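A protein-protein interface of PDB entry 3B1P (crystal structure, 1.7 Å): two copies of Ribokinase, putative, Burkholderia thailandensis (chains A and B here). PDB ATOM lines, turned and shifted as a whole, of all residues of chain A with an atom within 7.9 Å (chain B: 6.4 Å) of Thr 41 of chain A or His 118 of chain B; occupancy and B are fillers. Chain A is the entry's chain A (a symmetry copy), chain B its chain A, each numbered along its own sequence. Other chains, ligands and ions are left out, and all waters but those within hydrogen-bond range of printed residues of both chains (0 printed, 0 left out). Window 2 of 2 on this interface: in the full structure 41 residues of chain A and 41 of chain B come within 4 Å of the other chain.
The backbone NH (N) of Phe 117 of chain B is in hydrogen-bond range of the backbone carbonyl oxygen (O) of Phe 37 of chain A. The backbone carbonyl oxygen of Phe 117 of chain B is in hydrogen-bond range of the backbone NH of Val 39 of chain A. ND1 of His 118 of chain B lies within hydrogen-bond range of O of Val 39 of chain A, at 2.9 Å. OG1 of Thr 41 of chain A sits at hydrogen-bond distance from NE2 of His 118 of chain B (3.3 Å).
The backbone NH (N) of His 118 of chain B lies within hydrogen-bond range of the backbone carbonyl oxygen (O) of Gln 102 of chain B (2.8 Å). O of Ala 116 of chain B is in hydrogen-bond range of N of Met 104 of chain B.
Phe 37 of chain A touches Ala 116 of chain B (O to CA, 3.5 Å). CA of Leu 38 of chain A touches O of Phe 117 of chain B, 3.3 Å away. CB of Ala 116 of chain B touches CG1 of Val 39 of chain A, at 3.6 Å. Pro 40 of chain A touches His 118 of chain B. Met 42 of chain A touches Met 104 of chain B (SD to SD, 3.9 Å).
Of the printed residues of chain B, Phe 37 of chain A touches Ala 116 (3.5 Å) and Phe 117 (2.8 Å). Of the printed residues of chain B, Leu 38 of chain A touches Phe 117. Thr 41 of chain A touches just one residue of chain B: His 118. Of the printed residues of chain B, Met 42 of chain A touches Met 104. Printed residues of chain A within 4 Å of Phe 117 of chain B: Phe 37 (2.8 Å), Leu 38 (3.3 Å) and Val 39 (3.1 Å). His 118 of chain B touches just these residues of chain A: Val 39 (2.9 Å), Pro 40 (3.7 Å) and Thr 41 (3.3 Å). No residue of chain A comes within 4 Å of Pro 119 of chain B. The nearest printed residue of chain B that does not touch Thr 41 of chain A is Tyr 99 of chain B (7.2 Å). The nearest residue of chain A that does not touch His 118 of chain B is Leu 38 of chain A (5.3 Å).
Printed residues of chain B that touch a printed residue of chain A: Met 104, Ala 116, Phe 117 and His 118. Printed residues of chain A that touch a printed residue of chain B: Phe 37, Leu 38, Val 39, Pro 40, Thr 41 and Met 42. Among the printed residues, no Asp or Glu carboxylate lies within 4 Å of a Lys or Arg side-chain nitrogen of the other chain.
No position is printed for both chains.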
ATOM      1  N   ILE A  14     -33.031 -30.392 -12.645  1.00  0.00           N
ATOM      2  CA  ILE A  14     -31.876 -31.271 -12.919  1.00  0.00           C
ATOM      3  C   ILE A  14     -30.600 -30.680 -12.368  1.00  0.00           C
ATOM      4  O   ILE A  14     -30.250 -29.521 -12.670  1.00  0.00           O
ATOM      5  CB  ILE A  14     -31.767 -31.528 -14.470  1.00  0.00           C
ATOM      6  CG1 ILE A  14     -33.029 -32.255 -14.917  1.00  0.00           C
ATOM      7  CG2 ILE A  14     -30.480 -32.311 -14.757  1.00  0.00           C
ATOM      8  CD1 ILE A  14     -33.303 -32.184 -16.484  1.00  0.00           C
ATOM      9  N   PHE A  37     -21.191 -30.810  -5.012  1.00  0.00           N
ATOM     10  CA  PHE A  37     -20.743 -30.179  -6.251  1.00  0.00           C
ATOM     11  C   PHE A  37     -21.532 -28.913  -6.444  1.00  0.00           C
ATOM     12  O   PHE A  37     -22.717 -28.807  -6.071  1.00  0.00           O
ATOM     13  CB  PHE A  37     -20.852 -31.143  -7.468  1.00  0.00           C
ATOM     14  CG  PHE A  37     -22.233 -31.666  -7.748  1.00  0.00           C
ATOM     15  CD1 PHE A  37     -22.756 -32.762  -7.069  1.00  0.00           C
ATOM     16  CD2 PHE A  37     -23.009 -31.091  -8.728  1.00  0.00           C
ATOM     17  CE1 PHE A  37     -24.055 -33.231  -7.387  1.00  0.00           C
ATOM     18  CE2 PHE A  37     -24.277 -31.527  -9.000  1.00  0.00           C
ATOM     19  CZ  PHE A  37     -24.810 -32.615  -8.331  1.00  0.00           C
ATOM     20  N   LEU A  38     -20.851 -27.926  -7.024  1.00  0.00           N
ATOM     21  CA  LEU A  38     -21.431 -26.598  -7.154  1.00  0.00           C
ATOM     22  C   LEU A  38     -22.437 -26.584  -8.334  1.00  0.00           C
ATOM     23  O   LEU A  38     -22.217 -27.219  -9.393  1.00  0.00           O
ATOM     24  CB  LEU A  38     -20.306 -25.488  -7.064  1.00  0.00           C
ATOM     25  CG  LEU A  38     -19.438 -25.468  -5.740  1.00  0.00           C
ATOM     26  CD1 LEU A  38     -18.343 -24.359  -5.600  1.00  0.00           C
ATOM     27  CD2 LEU A  38     -20.277 -25.492  -4.399  1.00  0.00           C
ATOM     28  N   VAL A  39     -23.620 -25.988  -8.116  1.00  0.00           N
ATOM     29  CA  VAL A  39     -24.655 -25.882  -9.156  1.00  0.00           C
ATOM     30  C   VAL A  39     -25.050 -24.408  -9.314  1.00  0.00           C
ATOM     31  O   VAL A  39     -24.950 -23.652  -8.364  1.00  0.00           O
ATOM     32  CB  VAL A  39     -25.963 -26.722  -8.910  1.00  0.00           C
ATOM     33  CG1 VAL A  39     -25.719 -28.257  -9.103  1.00  0.00           C
ATOM     34  CG2 VAL A  39     -26.595 -26.427  -7.508  1.00  0.00           C
ATOM     35  N   PRO A  40     -25.536 -24.018 -10.510  1.00  0.00           N
ATOM     36  CA  PRO A  40     -26.092 -22.662 -10.639  1.00  0.00           C
ATOM     37  C   PRO A  40     -27.526 -22.628 -10.146  1.00  0.00           C
ATOM     38  O   PRO A  40     -28.047 -23.627  -9.659  1.00  0.00           O
ATOM     39  CB  PRO A  40     -26.019 -22.406 -12.161  1.00  0.00           C
ATOM     40  CG  PRO A  40     -26.224 -23.768 -12.789  1.00  0.00           C
ATOM     41  CD  PRO A  40     -25.416 -24.705 -11.817  1.00  0.00           C
ATOM     42  N   THR A  41     -28.194 -21.484 -10.280  1.00  0.00           N
ATOM     43  CA  THR A  41     -29.575 -21.364  -9.889  1.00  0.00           C
ATOM     44  C   THR A  41     -30.439 -22.468 -10.531  1.00  0.00           C
ATOM     45  O   THR A  41     -30.231 -22.802 -11.691  1.00  0.00           O
ATOM     46  CB  THR A  41     -30.082 -19.950 -10.266  1.00  0.00           C
ATOM     47  OG1 THR A  41     -29.277 -18.988  -9.559  1.00  0.00           O
ATOM     48  CG2 THR A  41     -31.534 -19.772  -9.892  1.00  0.00           C
ATOM     49  N   MET A  42     -31.386 -23.023  -9.769  1.00  0.00           N
ATOM     50  CA  MET A  42     -32.308 -24.036 -10.300  1.00  0.00           C
ATOM     51  C   MET A  42     -33.227 -23.475 -11.383  1.00  0.00           C
ATOM     52  O   MET A  42     -33.721 -22.364 -11.259  1.00  0.00           O
ATOM     53  CB  MET A  42     -33.165 -24.611  -9.178  1.00  0.00           C
ATOM     54  CG  MET A  42     -32.365 -25.317  -8.077  1.00  0.00           C
ATOM     55  SD  MET A  42     -33.284 -26.612  -7.189  1.00  0.00           S
ATOM     56  CE  MET A  42     -34.666 -25.738  -6.402  1.00  0.00           C
ATOM     57  N   ARG A  43     -33.426 -24.230 -12.454  1.00  0.00           N
ATOM     58  CA  ARG A  43     -34.416 -23.869 -13.477  1.00  0.00           C
ATOM     59  C   ARG A  43     -35.273 -25.062 -13.787  1.00  0.00           C
ATOM     60  O   ARG A  43     -34.778 -26.174 -13.953  1.00  0.00           O
ATOM     61  CB  ARG A  43     -33.801 -23.290 -14.772  1.00  0.00           C
ATOM     62  CG  ARG A  43     -32.477 -23.868 -15.224  1.00  0.00           C
ATOM     63  CD  ARG A  43     -31.945 -23.154 -16.480  1.00  0.00           C
ATOM     64  NE  ARG A  43     -32.664 -23.594 -17.686  1.00  0.00           N
ATOM     65  CZ  ARG A  43     -33.498 -22.847 -18.417  1.00  0.00           C
ATOM     66  NH1 ARG A  43     -33.724 -21.572 -18.110  1.00  0.00           N
ATOM     67  NH2 ARG A  43     -34.097 -23.382 -19.481  1.00  0.00           N
ATOM     68  N   ARG A  44     -36.571 -24.837 -13.837  1.00  0.00           N
ATOM     69  CA  ARG A  44     -37.504 -25.883 -14.088  1.00  0.00           C
ATOM     70  C   ARG A  44     -37.428 -26.132 -15.596  1.00  0.00           C
ATOM     71  O   ARG A  44     -37.206 -25.176 -16.358  1.00  0.00           O
ATOM     72  CB  ARG A  44     -38.866 -25.428 -13.642  1.00  0.00           C
ATOM     73  CG  ARG A  44     -39.879 -26.508 -13.583  1.00  0.00           C
ATOM     74  CD  ARG A  44     -41.247 -25.959 -13.167  1.00  0.00           C
ATOM     75  NE  ARG A  44     -41.902 -25.161 -14.225  1.00  0.00           N
ATOM     76  CZ  ARG A  44     -43.167 -24.727 -14.165  1.00  0.00           C
ATOM     77  NH1 ARG A  44     -43.916 -25.050 -13.122  1.00  0.00           N
ATOM     78  NH2 ARG A  44     -43.695 -24.002 -15.158  1.00  0.00           N
ATOM     79  N   TYR B  99     -27.555 -14.045  -1.879  1.00  0.00           N
ATOM     80  CA  TYR B  99     -28.426 -15.069  -1.291  1.00  0.00           C
ATOM     81  C   TYR B  99     -27.593 -16.019  -0.419  1.00  0.00           C
ATOM     82  O   TYR B  99     -26.422 -16.193  -0.657  1.00  0.00           O
ATOM     83  CB  TYR B  99     -29.075 -15.966  -2.359  1.00  0.00           C
ATOM     84  CG  TYR B  99     -30.158 -15.305  -3.113  1.00  0.00           C
ATOM     85  CD1 TYR B  99     -31.488 -15.615  -2.869  1.00  0.00           C
ATOM     86  CD2 TYR B  99     -29.852 -14.363  -4.097  1.00  0.00           C
ATOM     87  CE1 TYR B  99     -32.505 -14.988  -3.587  1.00  0.00           C
ATOM     88  CE2 TYR B  99     -30.865 -13.733  -4.801  1.00  0.00           C
ATOM     89  CZ  TYR B  99     -32.170 -14.064  -4.544  1.00  0.00           C
ATOM     90  OH  TYR B  99     -33.161 -13.436  -5.257  1.00  0.00           O
ATOM     91  N   SER B 100     -28.246 -16.587   0.578  1.00  0.00           N
ATOM     92  CA  SER B 100     -27.581 -17.556   1.488  1.00  0.00           C
ATOM     93  C   SER B 100     -27.352 -18.863   0.773  1.00  0.00           C
ATOM     94  O   SER B 100     -28.110 -19.229  -0.158  1.00  0.00           O
ATOM     95  CB  SER B 100     -28.509 -17.818   2.657  1.00  0.00           C
ATOM     96  OG  SER B 100     -28.741 -16.600   3.375  1.00  0.00           O
ATOM     97  N   ALA B 101     -26.337 -19.586   1.233  1.00  0.00           N
ATOM     98  CA  ALA B 101     -26.083 -20.957   0.699  1.00  0.00           C
ATOM     99  C   ALA B 101     -27.321 -21.845   0.716  1.00  0.00           C
ATOM    100  O   ALA B 101     -28.151 -21.792   1.629  1.00  0.00           O
ATOM    101  CB  ALA B 101     -24.950 -21.611   1.478  1.00  0.00           C
ATOM    102  N   GLN B 102     -27.477 -22.659  -0.327  1.00  0.00           N
ATOM    103  CA  GLN B 102     -28.579 -23.579  -0.428  1.00  0.00           C
ATOM    104  C   GLN B 102     -28.037 -24.962  -0.833  1.00  0.00           C
ATOM    105  O   GLN B 102     -27.264 -25.056  -1.790  1.00  0.00           O
ATOM    106  CB  GLN B 102     -29.570 -23.131  -1.516  1.00  0.00           C
ATOM    107  CG  GLN B 102     -30.935 -23.784  -1.391  1.00  0.00           C
ATOM    108  CD  GLN B 102     -32.009 -22.923  -0.670  1.00  0.00           C
ATOM    109  OE1 GLN B 102     -31.852 -21.700  -0.469  1.00  0.00           O
ATOM    110  NE2 GLN B 102     -33.123 -23.558  -0.318  1.00  0.00           N
ATOM    111  N   ALA B 103     -28.449 -26.008  -0.115  1.00  0.00           N
ATOM    112  CA  ALA B 103     -28.019 -27.379  -0.440  1.00  0.00           C
ATOM    113  C   ALA B 103     -29.244 -28.210  -0.853  1.00  0.00           C
ATOM    114  O   ALA B 103     -30.280 -28.216  -0.176  1.00  0.00           O
ATOM    115  CB  ALA B 103     -27.347 -28.019   0.784  1.00  0.00           C
ATOM    116  N   MET B 104     -29.154 -28.902  -1.997  1.00  0.00           N
ATOM    117  CA  MET B 104     -30.130 -29.916  -2.387  1.00  0.00           C
ATOM    118  C   MET B 104     -29.452 -31.242  -2.164  1.00  0.00           C
ATOM    119  O   MET B 104     -28.534 -31.632  -2.903  1.00  0.00           O
ATOM    120  CB  MET B 104     -30.458 -29.773  -3.887  1.00  0.00           C
ATOM    121  CG  MET B 104     -31.895 -29.866  -4.180  1.00  0.00           C
ATOM    122  SD  MET B 104     -32.803 -28.373  -3.728  1.00  0.00           S
ATOM    123  CE  MET B 104     -31.522 -27.067  -3.593  1.00  0.00           C
ATOM    124  N   ALA B 116     -26.125 -31.147  -4.391  1.00  0.00           N
ATOM    125  CA  ALA B 116     -25.956 -30.054  -5.334  1.00  0.00           C
ATOM    126  C   ALA B 116     -25.984 -28.779  -4.470  1.00  0.00           C
ATOM    127  O   ALA B 116     -26.981 -28.491  -3.824  1.00  0.00           O
ATOM    128  CB  ALA B 116     -27.106 -30.083  -6.296  1.00  0.00           C
ATOM    129  N   PHE B 117     -24.866 -28.085  -4.426  1.00  0.00           N
ATOM    130  CA  PHE B 117     -24.699 -26.942  -3.484  1.00  0.00           C
ATOM    131  C   PHE B 117     -24.576 -25.622  -4.235  1.00  0.00           C
ATOM    132  O   PHE B 117     -23.711 -25.464  -5.112  1.00  0.00           O
ATOM    133  CB  PHE B 117     -23.491 -27.209  -2.615  1.00  0.00           C
ATOM    134  CG  PHE B 117     -23.461 -26.409  -1.317  1.00  0.00           C
ATOM    135  CD1 PHE B 117     -24.214 -26.829  -0.217  1.00  0.00           C
ATOM    136  CD2 PHE B 117     -22.675 -25.262  -1.211  1.00  0.00           C
ATOM    137  CE1 PHE B 117     -24.170 -26.077   1.008  1.00  0.00           C
ATOM    138  CE2 PHE B 117     -22.612 -24.506  -0.001  1.00  0.00           C
ATOM    139  CZ  PHE B 117     -23.349 -24.916   1.096  1.00  0.00           C
ATOM    140  N   HIS B 118     -25.474 -24.695  -3.921  1.00  0.00           N
ATOM    141  CA  HIS B 118     -25.440 -23.355  -4.559  1.00  0.00           C
ATOM    142  C   HIS B 118     -24.937 -22.388  -3.460  1.00  0.00           C
ATOM    143  O   HIS B 118     -25.723 -22.037  -2.541  1.00  0.00           O
ATOM    144  CB  HIS B 118     -26.852 -23.055  -5.051  1.00  0.00           C
ATOM    145  CG  HIS B 118     -26.992 -21.792  -5.861  1.00  0.00           C
ATOM    146  ND1 HIS B 118     -26.160 -21.472  -6.916  1.00  0.00           N
ATOM    147  CD2 HIS B 118     -27.948 -20.831  -5.832  1.00  0.00           C
ATOM    148  CE1 HIS B 118     -26.557 -20.327  -7.455  1.00  0.00           C
ATOM    149  NE2 HIS B 118     -27.640 -19.921  -6.817  1.00  0.00           N
ATOM    150  N   PRO B 119     -23.641 -22.045  -3.495  1.00  0.00           N
ATOM    151  CA  PRO B 119     -22.981 -21.517  -2.284  1.00  0.00           C
ATOM    152  C   PRO B 119     -23.370 -20.089  -1.906  1.00  0.00           C
ATOM    153  O   PRO B 119     -23.295 -19.729  -0.722  1.00  0.00           O
ATOM    154  CB  PRO B 119     -21.514 -21.598  -2.600  1.00  0.00           C
ATOM    155  CG  PRO B 119     -21.443 -21.568  -4.118  1.00  0.00           C
ATOM    156  CD  PRO B 119     -22.664 -22.252  -4.594  1.00  0.00           C
ATOM    157  N   GLY B 120     -23.719 -19.265  -2.889  1.00  0.00           N
ATOM    158  CA  GLY B 120     -24.072 -17.882  -2.544  1.00  0.00           C
ATOM    159  C   GLY B 120     -23.048 -17.216  -1.652  1.00  0.00           C
ATOM    160  O   GLY B 120     -21.846 -17.174  -1.911  1.00  0.00           O
ATOM    161  N   ALA B 121     -23.548 -16.670  -0.541  1.00  0.00           N
ATOM    162  CA  ALA B 121     -22.713 -15.918   0.401  1.00  0.00           C
ATOM    163  C   ALA B 121     -21.592 -16.714   1.040  1.00  0.00           C
ATOM    164  O   ALA B 121     -20.590 -16.180   1.480  1.00  0.00           O
ATOM    165  CB  ALA B 121     -23.618 -15.287   1.528  1.00  0.00           C
